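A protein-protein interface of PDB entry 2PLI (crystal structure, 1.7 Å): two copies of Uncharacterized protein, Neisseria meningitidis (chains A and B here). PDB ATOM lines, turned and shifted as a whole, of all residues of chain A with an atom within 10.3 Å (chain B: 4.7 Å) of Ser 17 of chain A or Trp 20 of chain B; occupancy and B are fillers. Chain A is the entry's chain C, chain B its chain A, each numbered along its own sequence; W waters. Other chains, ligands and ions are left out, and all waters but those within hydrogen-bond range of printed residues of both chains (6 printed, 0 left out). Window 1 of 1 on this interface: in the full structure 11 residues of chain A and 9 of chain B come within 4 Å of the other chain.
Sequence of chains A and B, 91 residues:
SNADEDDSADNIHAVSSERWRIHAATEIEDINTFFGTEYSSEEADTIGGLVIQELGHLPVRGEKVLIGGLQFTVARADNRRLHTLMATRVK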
ATOM      1  N   ASP A  10      20.598 -23.152   3.371  1.00  0.00           N
ATOM      2  CA  ASP A  10      19.838 -22.019   3.977  1.00  0.00           C
ATOM      3  C   ASP A  10      20.743 -21.016   4.734  1.00  0.00           C
ATOM      4  O   ASP A  10      21.407 -21.336   5.753  1.00  0.00           O
ATOM      5  CB  ASP A  10      18.739 -22.577   4.889  1.00  0.00           C
ATOM      6  CG  ASP A  10      19.270 -23.589   5.847  1.00  0.00           C
ATOM      7  OD1 ASP A  10      20.259 -24.283   5.523  1.00  0.00           O
ATOM      8  OD2 ASP A  10      18.727 -23.679   6.911  1.00  0.00           O
ATOM      9  N   ILE A  12      19.454 -18.617   6.230  1.00  0.00           N
ATOM     10  CA  ILE A  12      18.641 -18.316   7.397  1.00  0.00           C
ATOM     11  C   ILE A  12      18.043 -19.663   7.857  1.00  0.00           C
ATOM     12  O   ILE A  12      17.185 -20.263   7.183  1.00  0.00           O
ATOM     13  CB  ILE A  12      17.492 -17.309   7.116  1.00  0.00           C
ATOM     14  CG1 ILE A  12      18.058 -16.008   6.514  1.00  0.00           C
ATOM     15  CG2 ILE A  12      16.725 -17.020   8.416  1.00  0.00           C
ATOM     16  CD1 ILE A  12      16.985 -15.035   6.015  1.00  0.00           C
ATOM     17  N   HIS A  13      18.567 -20.132   8.970  1.00  0.00           N
ATOM     18  CA  HIS A  13      18.251 -21.450   9.539  1.00  0.00           C
ATOM     19  C   HIS A  13      17.547 -21.246  10.864  1.00  0.00           C
ATOM     20  O   HIS A  13      18.102 -20.589  11.798  1.00  0.00           O
ATOM     21  CB  HIS A  13      19.563 -22.201   9.775  1.00  0.00           C
ATOM     22  CG  HIS A  13      19.420 -23.445  10.570  1.00  0.00           C
ATOM     23  ND1 HIS A  13      19.274 -24.694   9.991  1.00  0.00           N
ATOM     24  CD2 HIS A  13      19.439 -23.638  11.911  1.00  0.00           C
ATOM     25  CE1 HIS A  13      19.183 -25.599  10.960  1.00  0.00           C
ATOM     26  NE2 HIS A  13      19.254 -24.980  12.131  1.00  0.00           N
ATOM     27  N   ALA A  14      16.361 -21.813  11.019  1.00  0.00           N
ATOM     28  CA  ALA A  14      15.665 -21.767  12.338  1.00  0.00           C
ATOM     29  C   ALA A  14      16.277 -22.781  13.290  1.00  0.00           C
ATOM     30  O   ALA A  14      16.205 -23.997  13.054  1.00  0.00           O
ATOM     31  CB  ALA A  14      14.183 -22.024  12.224  1.00  0.00           C
ATOM     32  N   VAL A  15      16.921 -22.271  14.330  1.00  0.00           N
ATOM     33  CA  VAL A  15      17.391 -23.079  15.441  1.00  0.00           C
ATOM     34  C   VAL A  15      16.194 -23.585  16.264  1.00  0.00           C
ATOM     35  O   VAL A  15      16.117 -24.772  16.651  1.00  0.00           O
ATOM     36  CB  VAL A  15      18.400 -22.260  16.284  1.00  0.00           C
ATOM     37  CG1 VAL A  15      18.685 -22.918  17.588  1.00  0.00           C
ATOM     38  CG2 VAL A  15      19.735 -22.065  15.493  1.00  0.00           C
ATOM     39  N   SER A  16      15.249 -22.680  16.494  1.00  0.00           N
ATOM     40  CA  SER A  16      13.974 -22.948  17.119  1.00  0.00           C
ATOM     41  C   SER A  16      12.956 -22.029  16.424  1.00  0.00           C
ATOM     42  O   SER A  16      13.313 -21.258  15.520  1.00  0.00           O
ATOM     43  CB  SER A  16      14.048 -22.753  18.648  1.00  0.00           C
ATOM     44  OG  SER A  16      14.419 -21.422  18.969  1.00  0.00           O
ATOM     45  N   SER A  17      11.699 -22.115  16.811  1.00  0.00           N
ATOM     46  CA  SER A  17      10.635 -21.449  16.048  1.00  0.00           C
ATOM     47  C   SER A  17      10.807 -19.938  16.015  1.00  0.00           C
ATOM     48  O   SER A  17      10.365 -19.312  15.061  1.00  0.00           O
ATOM     49  CB  SER A  17       9.257 -21.855  16.555  1.00  0.00           C
ATOM     50  OG  SER A  17       9.042 -21.372  17.842  1.00  0.00           O
ATOM     51  N   GLU A  18      11.445 -19.363  17.063  1.00  0.00           N
ATOM     52  CA  GLU A  18      11.604 -17.937  17.189  1.00  0.00           C
ATOM     53  C   GLU A  18      13.054 -17.468  17.279  1.00  0.00           C
ATOM     54  O   GLU A  18      13.304 -16.377  17.782  1.00  0.00           O
ATOM     55  CB  GLU A  18      10.816 -17.464  18.428  1.00  0.00           C
ATOM     56  CG  GLU A  18       9.308 -17.567  18.255  1.00  0.00           C
ATOM     57  CD  GLU A  18       8.808 -16.837  16.985  1.00  0.00           C
ATOM     58  OE1 GLU A  18       9.042 -15.597  16.836  1.00  0.00           O
ATOM     59  OE2 GLU A  18       8.207 -17.513  16.120  1.00  0.00           O
ATOM     60  N   ARG A  19      13.997 -18.282  16.807  1.00  0.00           N
ATOM     61  CA  ARG A  19      15.402 -17.926  16.844  1.00  0.00           C
ATOM     62  C   ARG A  19      16.098 -18.493  15.651  1.00  0.00           C
ATOM     63  O   ARG A  19      15.954 -19.689  15.348  1.00  0.00           O
ATOM     64  CB  ARG A  19      16.029 -18.434  18.137  1.00  0.00           C
ATOM     65  CG  ARG A  19      17.470 -17.972  18.397  1.00  0.00           C
ATOM     66  CD  ARG A  19      17.803 -17.941  19.892  1.00  0.00           C
ATOM     67  NE  ARG A  19      19.230 -17.757  20.196  1.00  0.00           N
ATOM     68  CZ  ARG A  19      20.136 -18.745  20.240  1.00  0.00           C
ATOM     69  NH1 ARG A  19      21.401 -18.467  20.534  1.00  0.00           N
ATOM     70  NH2 ARG A  19      19.797 -20.018  20.008  1.00  0.00           N
ATOM     71  N   TRP A  20      16.825 -17.632  14.939  1.00  0.00           N
ATOM     72  CA  TRP A  20      17.396 -17.953  13.635  1.00  0.00           C
ATOM     73  C   TRP A  20      18.878 -17.716  13.571  1.00  0.00           C
ATOM     74  O   TRP A  20      19.360 -16.685  14.027  1.00  0.00           O
ATOM     75  CB  TRP A  20      16.734 -17.107  12.510  1.00  0.00           C
ATOM     76  CG  TRP A  20      15.268 -17.293  12.495  1.00  0.00           C
ATOM     77  CD1 TRP A  20      14.600 -18.282  11.888  1.00  0.00           C
ATOM     78  CD2 TRP A  20      14.280 -16.496  13.181  1.00  0.00           C
ATOM     79  NE1 TRP A  20      13.237 -18.157  12.108  1.00  0.00           N
ATOM     80  CE2 TRP A  20      13.025 -17.070  12.908  1.00  0.00           C
ATOM     81  CE3 TRP A  20      14.338 -15.377  14.020  1.00  0.00           C
ATOM     82  CZ2 TRP A  20      11.854 -16.571  13.420  1.00  0.00           C
ATOM     83  CZ3 TRP A  20      13.161 -14.890  14.537  1.00  0.00           C
ATOM     84  CH2 TRP A  20      11.941 -15.471  14.218  1.00  0.00           C
ATOM     85  N   ARG A  21      19.585 -18.677  12.989  1.00  0.00           N
ATOM     86  CA  ARG A  21      21.020 -18.590  12.757  1.00  0.00           C
ATOM     87  C   ARG A  21      21.193 -18.076  11.329  1.00  0.00           C
ATOM     88  O   ARG A  21      20.677 -18.683  10.374  1.00  0.00           O
ATOM     89  CB  ARG A  21      21.696 -19.943  12.890  1.00  0.00           C
ATOM     90  CG  ARG A  21      23.136 -19.976  12.383  1.00  0.00           C
ATOM     91  CD  ARG A  21      23.776 -21.308  12.729  1.00  0.00           C
ATOM     92  NE  ARG A  21      23.335 -22.396  11.874  1.00  0.00           N
ATOM     93  CZ  ARG A  21      22.903 -23.580  12.293  1.00  0.00           C
ATOM     94  NH1 ARG A  21      22.790 -23.885  13.569  1.00  0.00           N
ATOM     95  NH2 ARG A  21      22.609 -24.508  11.403  1.00  0.00           N
ATOM     96  N   PHE A  34      12.305 -13.217   4.011  1.00  0.00           N
ATOM     97  CA  PHE A  34      12.040 -14.240   5.044  1.00  0.00           C
ATOM     98  C   PHE A  34      11.236 -13.661   6.202  1.00  0.00           C
ATOM     99  O   PHE A  34      10.331 -14.319   6.737  1.00  0.00           O
ATOM    100  CB  PHE A  34      13.362 -14.746   5.568  1.00  0.00           C
ATOM    101  CG  PHE A  34      13.242 -15.895   6.541  1.00  0.00           C
ATOM    102  CD1 PHE A  34      13.247 -17.180   6.068  1.00  0.00           C
ATOM    103  CD2 PHE A  34      13.198 -15.673   7.934  1.00  0.00           C
ATOM    104  CE1 PHE A  34      13.174 -18.257   6.951  1.00  0.00           C
ATOM    105  CE2 PHE A  34      13.159 -16.763   8.834  1.00  0.00           C
ATOM    106  CZ  PHE A  34      13.156 -18.032   8.338  1.00  0.00           C
ATOM    107  N   PHE A  35      11.570 -12.425   6.612  1.00  0.00           N
ATOM    108  CA  PHE A  35      10.980 -11.817   7.811  1.00  0.00           C
ATOM    109  C   PHE A  35       9.849 -10.800   7.596  1.00  0.00           C
ATOM    110  O   PHE A  35       9.154 -10.421   8.554  1.00  0.00           O
ATOM    111  CB  PHE A  35      12.079 -11.123   8.625  1.00  0.00           C
ATOM    112  CG  PHE A  35      13.049 -12.093   9.300  1.00  0.00           C
ATOM    113  CD1 PHE A  35      12.641 -12.825  10.399  1.00  0.00           C
ATOM    114  CD2 PHE A  35      14.322 -12.284   8.837  1.00  0.00           C
ATOM    115  CE1 PHE A  35      13.505 -13.706  11.035  1.00  0.00           C
ATOM    116  CE2 PHE A  35      15.210 -13.133   9.496  1.00  0.00           C
ATOM    117  CZ  PHE A  35      14.781 -13.869  10.567  1.00  0.00           C
ATOM    118  N   LEU A  70      13.592  -6.769  14.852  1.00  0.00           N
ATOM    119  CA  LEU A  70      14.461  -7.944  15.088  1.00  0.00           C
ATOM    120  C   LEU A  70      15.655  -7.527  15.929  1.00  0.00           C
ATOM    121  O   LEU A  70      16.221  -6.443  15.735  1.00  0.00           O
ATOM    122  CB  LEU A  70      14.970  -8.561  13.786  1.00  0.00           C
ATOM    123  CG  LEU A  70      13.962  -9.157  12.771  1.00  0.00           C
ATOM    124  CD1 LEU A  70      14.630  -9.581  11.491  1.00  0.00           C
ATOM    125  CD2 LEU A  70      13.293 -10.342  13.441  1.00  0.00           C
ATOM    126  N   ALA A  87      19.293 -14.200  15.274  1.00  0.00           N
ATOM    127  CA  ALA A  87      18.185 -13.235  15.312  1.00  0.00           C
ATOM    128  C   ALA A  87      17.048 -13.740  16.201  1.00  0.00           C
ATOM    129  O   ALA A  87      16.741 -14.935  16.201  1.00  0.00           O
ATOM    130  CB  ALA A  87      17.653 -12.976  13.916  1.00  0.00           C
ATOM    131  N   THR A  88      16.405 -12.798  16.884  1.00  0.00           N
ATOM    132  CA  THR A  88      15.116 -13.041  17.542  1.00  0.00           C
ATOM    133  C   THR A  88      14.218 -11.827  17.291  1.00  0.00           C
ATOM    134  O   THR A  88      14.704 -10.798  16.874  1.00  0.00           O
ATOM    135  CB  THR A  88      15.301 -13.242  19.043  1.00  0.00           C
ATOM    136  OG1 THR A  88      15.878 -12.064  19.618  1.00  0.00           O
ATOM    137  CG2 THR A  88      16.181 -14.463  19.313  1.00  0.00           C
ATOM    138  N   ARG A  89      12.905 -11.969  17.499  1.00  0.00           N
ATOM    139  CA  ARG A  89      11.967 -10.852  17.353  1.00  0.00           C
ATOM    140  C   ARG A  89      11.961 -10.038  18.657  1.00  0.00           C
ATOM    141  O   ARG A  89      12.096 -10.595  19.753  1.00  0.00           O
ATOM    142  CB  ARG A  89      10.550 -11.361  16.957  1.00  0.00           C
ATOM    143  CG  ARG A  89      10.440 -11.845  15.479  1.00  0.00           C
ATOM    144  CD  ARG A  89       8.975 -12.011  14.962  1.00  0.00           C
ATOM    145  NE  ARG A  89       8.885 -12.292  13.511  1.00  0.00           N
ATOM    146  CZ  ARG A  89       8.990 -11.405  12.519  1.00  0.00           C
ATOM    147  NH1 ARG A  89       9.211 -10.104  12.755  1.00  0.00           N
ATOM    148  NH2 ARG A  89       8.870 -11.817  11.249  1.00  0.00           N
ATOM    149  N   ILE B  12      12.976 -29.706  10.386  1.00  0.00           N
ATOM    150  CA  ILE B  12      11.992 -28.642  10.601  1.00  0.00           C
ATOM    151  C   ILE B  12      12.541 -27.412   9.922  1.00  0.00           C
ATOM    152  O   ILE B  12      13.446 -26.779  10.471  1.00  0.00           O
ATOM    153  CB  ILE B  12      11.745 -28.338  12.106  1.00  0.00           C
ATOM    154  CG1 ILE B  12      11.342 -29.584  12.891  1.00  0.00           C
ATOM    155  CG2 ILE B  12      10.675 -27.243  12.272  1.00  0.00           C
ATOM    156  CD1 ILE B  12      11.209 -29.379  14.393  1.00  0.00           C
ATOM    157  N   HIS B  13      12.024 -27.094   8.740  1.00  0.00           N
ATOM    158  CA  HIS B  13      12.640 -26.092   7.867  1.00  0.00           C
ATOM    159  C   HIS B  13      11.782 -24.875   7.793  1.00  0.00           C
ATOM    160  O   HIS B  13      10.652 -24.962   7.370  1.00  0.00           O
ATOM    161  CB  HIS B  13      12.776 -26.662   6.486  1.00  0.00           C
ATOM    162  CG  HIS B  13      13.439 -25.733   5.547  1.00  0.00           C
ATOM    163  ND1 HIS B  13      14.700 -25.217   5.790  1.00  0.00           N
ATOM    164  CD2 HIS B  13      13.029 -25.225   4.368  1.00  0.00           C
ATOM    165  CE1 HIS B  13      15.012 -24.390   4.804  1.00  0.00           C
ATOM    166  NE2 HIS B  13      14.013 -24.383   3.937  1.00  0.00           N
ATOM    167  N   ALA B  14      12.297 -23.732   8.195  1.00  0.00           N
ATOM    168  CA  ALA B  14      11.499 -22.527   8.099  1.00  0.00           C
ATOM    169  C   ALA B  14      11.506 -22.055   6.653  1.00  0.00           C
ATOM    170  O   ALA B  14      12.549 -21.626   6.167  1.00  0.00           O
ATOM    171  CB  ALA B  14      12.056 -21.435   9.009  1.00  0.00           C
ATOM    172  N   VAL B  15      10.355 -22.071   6.005  1.00  0.00           N
ATOM    173  CA  VAL B  15      10.241 -21.585   4.649  1.00  0.00           C
ATOM    174  C   VAL B  15      10.118 -20.068   4.626  1.00  0.00           C
ATOM    175  O   VAL B  15      10.417 -19.407   3.605  1.00  0.00           O
ATOM    176  CB  VAL B  15       9.080 -22.257   3.892  1.00  0.00           C
ATOM    177  CG1 VAL B  15       9.297 -23.773   3.805  1.00  0.00           C
ATOM    178  CG2 VAL B  15       7.759 -21.974   4.521  1.00  0.00           C
ATOM    179  N   SER B  17       9.646 -16.856   8.194  1.00  0.00           N
ATOM    180  CA  SER B  17       9.826 -16.761   9.637  1.00  0.00           C
ATOM    181  C   SER B  17       8.733 -17.462  10.437  1.00  0.00           C
ATOM    182  O   SER B  17       9.014 -17.946  11.534  1.00  0.00           O
ATOM    183  CB  SER B  17      10.007 -15.315  10.102  1.00  0.00           C
ATOM    184  OG  SER B  17       8.801 -14.590   9.982  1.00  0.00           O
ATOM    185  N   GLU B  18       7.498 -17.511   9.905  1.00  0.00           N
ATOM    186  CA  GLU B  18       6.385 -18.133  10.621  1.00  0.00           C
ATOM    187  C   GLU B  18       5.691 -19.334   9.950  1.00  0.00           C
ATOM    188  O   GLU B  18       4.538 -19.636  10.239  1.00  0.00           O
ATOM    189  CB  GLU B  18       5.364 -17.089  11.054  1.00  0.00           C
ATOM    190  CG  GLU B  18       5.872 -16.152  12.169  1.00  0.00           C
ATOM    191  CD  GLU B  18       6.110 -16.884  13.510  1.00  0.00           C
ATOM    192  OE1 GLU B  18       5.142 -17.516  14.063  1.00  0.00           O
ATOM    193  OE2 GLU B  18       7.284 -16.854  13.985  1.00  0.00           O
ATOM    194  N   ARG B  19       6.428 -20.065   9.135  1.00  0.00           N
ATOM    195  CA  ARG B  19       5.873 -21.238   8.465  1.00  0.00           C
ATOM    196  C   ARG B  19       6.987 -22.239   8.276  1.00  0.00           C
ATOM    197  O   ARG B  19       8.085 -21.872   7.900  1.00  0.00           O
ATOM    198  CB  ARG B  19       5.325 -20.813   7.116  1.00  0.00           C
ATOM    199  CG  ARG B  19       4.351 -21.742   6.553  1.00  0.00           C
ATOM    200  CD  ARG B  19       3.307 -20.891   5.803  1.00  0.00           C
ATOM    201  NE  ARG B  19       2.566 -21.740   4.932  1.00  0.00           N
ATOM    202  CZ  ARG B  19       2.858 -21.964   3.665  1.00  0.00           C
ATOM    203  NH1 ARG B  19       3.835 -21.321   3.034  1.00  0.00           N
ATOM    204  NH2 ARG B  19       2.106 -22.804   3.036  1.00  0.00           N
ATOM    205  N   TRP B  20       6.683 -23.500   8.555  1.00  0.00           N
ATOM    206  CA  TRP B  20       7.681 -24.538   8.581  1.00  0.00           C
ATOM    207  C   TRP B  20       7.282 -25.773   7.794  1.00  0.00           C
ATOM    208  O   TRP B  20       6.168 -26.286   7.957  1.00  0.00           O
ATOM    209  CB  TRP B  20       7.943 -24.962  10.041  1.00  0.00           C
ATOM    210  CG  TRP B  20       8.303 -23.819  10.898  1.00  0.00           C
ATOM    211  CD1 TRP B  20       9.547 -23.320  11.097  1.00  0.00           C
ATOM    212  CD2 TRP B  20       7.413 -22.991  11.662  1.00  0.00           C
ATOM    213  NE1 TRP B  20       9.502 -22.220  11.920  1.00  0.00           N
ATOM    214  CE2 TRP B  20       8.199 -21.982  12.262  1.00  0.00           C
ATOM    215  CE3 TRP B  20       6.033 -22.984  11.892  1.00  0.00           C
ATOM    216  CZ2 TRP B  20       7.650 -20.998  13.079  1.00  0.00           C
ATOM    217  CZ3 TRP B  20       5.483 -21.965  12.705  1.00  0.00           C
ATOM    218  CH2 TRP B  20       6.296 -21.010  13.284  1.00  0.00           C
ATOM    219  N   ARG B  21       8.202 -26.290   6.991  1.00  0.00           N
ATOM    220  CA  ARG B  21       7.975 -27.557   6.333  1.00  0.00           C
ATOM    221  C   ARG B  21       8.642 -28.622   7.177  1.00  0.00           C
ATOM    222  O   ARG B  21       9.845 -28.488   7.494  1.00  0.00           O
ATOM    223  CB  ARG B  21       8.560 -27.558   4.928  1.00  0.00           C
ATOM    224  CG  ARG B  21       8.179 -28.852   4.195  1.00  0.00           C
ATOM    225  CD  ARG B  21       8.782 -28.909   2.784  1.00  0.00           C
ATOM    226  NE  ARG B  21       8.396 -27.791   1.957  1.00  0.00           N
ATOM    227  CZ  ARG B  21       9.218 -26.813   1.566  1.00  0.00           C
ATOM    228  NH1 ARG B  21      10.510 -26.797   1.927  1.00  0.00           N
ATOM    229  NH2 ARG B  21       8.747 -25.836   0.815  1.00  0.00           N
ATOM    230  N   ILE B  22       7.885 -29.645   7.568  1.00  0.00           N
ATOM    231  CA  ILE B  22       8.385 -30.599   8.563  1.00  0.00           C
ATOM    232  C   ILE B  22       8.348 -32.041   8.033  1.00  0.00           C
ATOM    233  O   ILE B  22       7.307 -32.518   7.576  1.00  0.00           O
ATOM    234  CB  ILE B  22       7.515 -30.521   9.864  1.00  0.00           C
ATOM    235  CG1 ILE B  22       7.515 -29.102  10.437  1.00  0.00           C
ATOM    236  CG2 ILE B  22       8.014 -31.516  10.931  1.00  0.00           C
ATOM    237  CD1 ILE B  22       6.696 -28.918  11.716  1.00  0.00           C
ATOM    238  N   PHE B  34      11.667 -27.436  19.547  1.00  0.00           N
ATOM    239  CA  PHE B  34      11.625 -26.401  18.519  1.00  0.00           C
ATOM    240  C   PHE B  34      10.531 -25.392  18.765  1.00  0.00           C
ATOM    241  O   PHE B  34      10.752 -24.164  18.627  1.00  0.00           O
ATOM    242  CB  PHE B  34      11.514 -27.037  17.141  1.00  0.00           C
ATOM    243  CG  PHE B  34      11.632 -26.045  16.002  1.00  0.00           C
ATOM    244  CD1 PHE B  34      12.880 -25.850  15.359  1.00  0.00           C
ATOM    245  CD2 PHE B  34      10.530 -25.335  15.533  1.00  0.00           C
ATOM    246  CE1 PHE B  34      13.011 -24.990  14.300  1.00  0.00           C
ATOM    247  CE2 PHE B  34      10.654 -24.477  14.485  1.00  0.00           C
ATOM    248  CZ  PHE B  34      11.894 -24.256  13.878  1.00  0.00           C
ATOM    249  N   PHE B  35       9.358 -25.875  19.169  1.00  0.00           N
ATOM    250  CA  PHE B  35       8.187 -25.039  19.261  1.00  0.00           C
ATOM    251  C   PHE B  35       7.781 -24.671  20.668  1.00  0.00           C
ATOM    252  O   PHE B  35       6.914 -23.829  20.849  1.00  0.00           O
ATOM    253  CB  PHE B  35       6.989 -25.720  18.599  1.00  0.00           C
ATOM    254  CG  PHE B  35       7.075 -25.763  17.109  1.00  0.00           C
ATOM    255  CD1 PHE B  35       6.874 -24.622  16.356  1.00  0.00           C
ATOM    256  CD2 PHE B  35       7.375 -26.942  16.448  1.00  0.00           C
ATOM    257  CE1 PHE B  35       6.989 -24.652  14.992  1.00  0.00           C
ATOM    258  CE2 PHE B  35       7.475 -26.984  15.082  1.00  0.00           C
ATOM    259  CZ  PHE B  35       7.305 -25.843  14.344  1.00  0.00           C
ATOM    260  N   LEU B  85       4.731 -32.359   6.302  1.00  0.00           N
ATOM    261  CA  LEU B  85       3.698 -31.464   6.845  1.00  0.00           C
ATOM    262  C   LEU B  85       4.140 -30.011   6.646  1.00  0.00           C
ATOM    263  O   LEU B  85       5.324 -29.726   6.593  1.00  0.00           O
ATOM    264  CB  LEU B  85       3.551 -31.713   8.342  1.00  0.00           C
ATOM    265  CG  LEU B  85       3.114 -33.127   8.751  1.00  0.00           C
ATOM    266  CD1 LEU B  85       3.408 -33.369  10.176  1.00  0.00           C
ATOM    267  CD2 LEU B  85       1.604 -33.302   8.411  1.00  0.00           C
ATOM    268  N   MET B  86       3.170 -29.111   6.546  1.00  0.00           N
ATOM    269  CA  MET B  86       3.398 -27.657   6.647  1.00  0.00           C
ATOM    270  C   MET B  86       2.700 -27.182   7.889  1.00  0.00           C
ATOM    271  O   MET B  86       1.493 -27.431   8.064  1.00  0.00           O
ATOM    272  CB  MET B  86       2.832 -26.945   5.424  1.00  0.00           C
ATOM    273  CG  MET B  86       3.129 -25.464   5.358  1.00  0.00           C
ATOM    274  SD  MET B  86       5.032 -25.139   5.009  1.00  0.00           S
ATOM    275  CE  MET B  86       5.092 -25.194   3.094  1.00  0.00           C
ATOM    276  N   ALA B  87       3.441 -26.496   8.748  1.00  0.00           N
ATOM    277  CA  ALA B  87       2.895 -26.037  10.033  1.00  0.00           C
ATOM    278  C   ALA B  87       2.902 -24.536  10.116  1.00  0.00           C
ATOM    279  O   ALA B  87       3.808 -23.866   9.573  1.00  0.00           O
ATOM    280  CB  ALA B  87       3.683 -26.583  11.165  1.00  0.00           C
ATOM    281  N   THR B  88       1.887 -24.001  10.806  1.00  0.00           N
ATOM    282  CA  THR B  88       1.851 -22.582  11.152  1.00  0.00           C
ATOM    283  C   THR B  88       1.239 -22.513  12.538  1.00  0.00           C
ATOM    284  O   THR B  88       0.578 -23.460  12.992  1.00  0.00           O
ATOM    285  CB  THR B  88       1.032 -21.761  10.163  1.00  0.00           C
ATOM    286  OG1 THR B  88      -0.288 -22.294  10.073  1.00  0.00           O
ATOM    287  CG2 THR B  88       1.678 -21.772   8.809  1.00  0.00           C
ATOM    288  N   ARG B  89       1.473 -21.385  13.216  1.00  0.00           N
ATOM    289  CA  ARG B  89       0.876 -21.131  14.531  1.00  0.00           C
ATOM    290  C   ARG B  89      -0.596 -20.723  14.418  1.00  0.00           C
ATOM    291  O   ARG B  89      -0.958 -19.877  13.597  1.00  0.00           O
ATOM    292  CB  ARG B  89       1.679 -20.046  15.278  1.00  0.00           C
ATOM    293  CG  ARG B  89       3.028 -20.560  15.816  1.00  0.00           C
ATOM    294  CD  ARG B  89       3.649 -19.657  16.903  1.00  0.00           C
ATOM    295  NE  ARG B  89       4.896 -20.223  17.475  1.00  0.00           N
ATOM    296  CZ  ARG B  89       4.978 -21.237  18.347  1.00  0.00           C
ATOM    297  NH1 ARG B  89       3.899 -21.870  18.772  1.00  0.00           N
ATOM    298  NH2 ARG B  89       6.165 -21.639  18.809  1.00  0.00           N
HETATM  299  O   HOH W   1      15.286 -22.111   6.899  1.00  0.00           O
HETATM  300  O   HOH W   2       7.462 -13.870   7.654  1.00  0.00           O
HETATM  301  O   HOH W   3      15.124 -23.492   9.050  1.00  0.00           O
HETATM  302  O   HOH W   4      10.196 -21.651  20.361  1.00  0.00           O
HETATM  303  O   HOH W   5      15.739 -25.781  11.134  1.00  0.00           O
HETATM  304  O   HOH W   6      10.942 -19.822  12.274  1.00  0.00           O
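N of Ser 17 of chain B sits at hydrogen-bond distance from O of Phe 34 of chain A (3.0 Å).
The side-chain hydroxyl of Ser 17 of chain B is in hydrogen-bond range of the guanidinium group of Arg 89 of chain A, 3.0 Å away.
The side-chain carboxylate (OE2) of Glu 18 of chain B lies close to the side-chain carboxylate (OE2) of Glu 18 of chain A.
The backbone carbonyl oxygen of Phe 34 of chain B lies within hydrogen-bond range of the backbone NH of Ser 17 of chain A, 2.9 Å away.
The side-chain hydroxyl (OG) of Ser 17 of chain A lies within hydrogen-bond range of the guanidinium group (NH2) of Arg 89 of chain B (3.0 Å).
The backbone carbonyl oxygen (O) of Trp 20 of chain A is in hydrogen-bond range of the backbone NH (N) of Ala 87 of chain A (2.8 Å).
O of Phe 35 of chain A lies within hydrogen-bond range of NH2 of Arg 89 of chain A (3.0 Å).
Among the printed residues, pairs that only touch across the chains: Ala 14 of chain A with Ala 14 of chain B (3.9 Å), Ala 14 of chain A with Phe 34 of chain B (3.6 Å), Val 15 of chain A with Phe 34 of chain B (3.6 Å), Ser 16 of chain A with Phe 34 of chain B (3.5 Å), Ser 17 of chain A with Trp 20 of chain B (3.8 Å), Ser 17 of chain A with Phe 35 of chain B (3.7 Å), Trp 20 of chain A with Ser 17 of chain B (3.7 Å), Phe 34 of chain A with Ala 14 of chain B (3.5 Å) and Phe 35 of chain A with Ser 17 of chain B (3.6 Å).
Of the printed residues of chain B, Arg 89 of chain A touches Ser 17 (3.0 Å).
Ala 14 of chain B touches two residues of chain A.
Of chain A, only Ser 17 (3.8 Å) comes within 4 Å of Trp 20 of chain B.
Printed residues of chain A within 4 Å of Phe 34 of chain B: Ala 14 (3.6 Å), Val 15 (3.6 Å), Ser 16 (3.5 Å) and Ser 17 (2.9 Å).
No residue of chain A comes within 4 Å of Ala 87 of chain B.
Of the printed residues of chain A, Arg 89 of chain B touches Ser 17 (3.0 Å).
The nearest residue of chain A that does not touch Trp 20 of chain B is Glu 18 of chain A (4.7 Å).
The nearest printed residue of chain B that does not touch Arg 89 of chain A is Glu 18 of chain B (4.9 Å).
Hydrophobic or aromatic side chains of chain B that line the printed part of chain A: Ala 14, Trp 20, Phe 34 and Phe 35.
Of the 17 printed residues of chain A, 9 touch a printed residue of chain B.
Printed residues of chain A that touch a printed residue of chain B: Ala 14, Val 15, Ser 16, Ser 17, Glu 18, Trp 20, Phe 34, Phe 35 and Arg 89.
Along chain A the printed residues that touch a printed residue of chain B span positions 14 to 89.
Among the printed residues, 14 pairs touch across the chains.
Among the printed residues, no Asp or Glu carboxylate lies within 4 Å of a Lys or Arg side-chain nitrogen of the other chain.
Ser 17 of chain A touches Phe 35 of chain B, and with the chains exchanged Phe 35 of chain A touches Ser 17 of chain B.
Of the 14 pairs that touch across the chains among the printed residues, 12 have their exchanged pair printed and touching as well.
Water W6 lies within hydrogen-bond range of O of Ser 17 of chain B (2.8 Å), NE1 of Trp 20 of chain B (2.8 Å), NE1 of Trp 20 of chain A (2.8 Å) and O of Ser 17 of chain A (2.9 Å).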
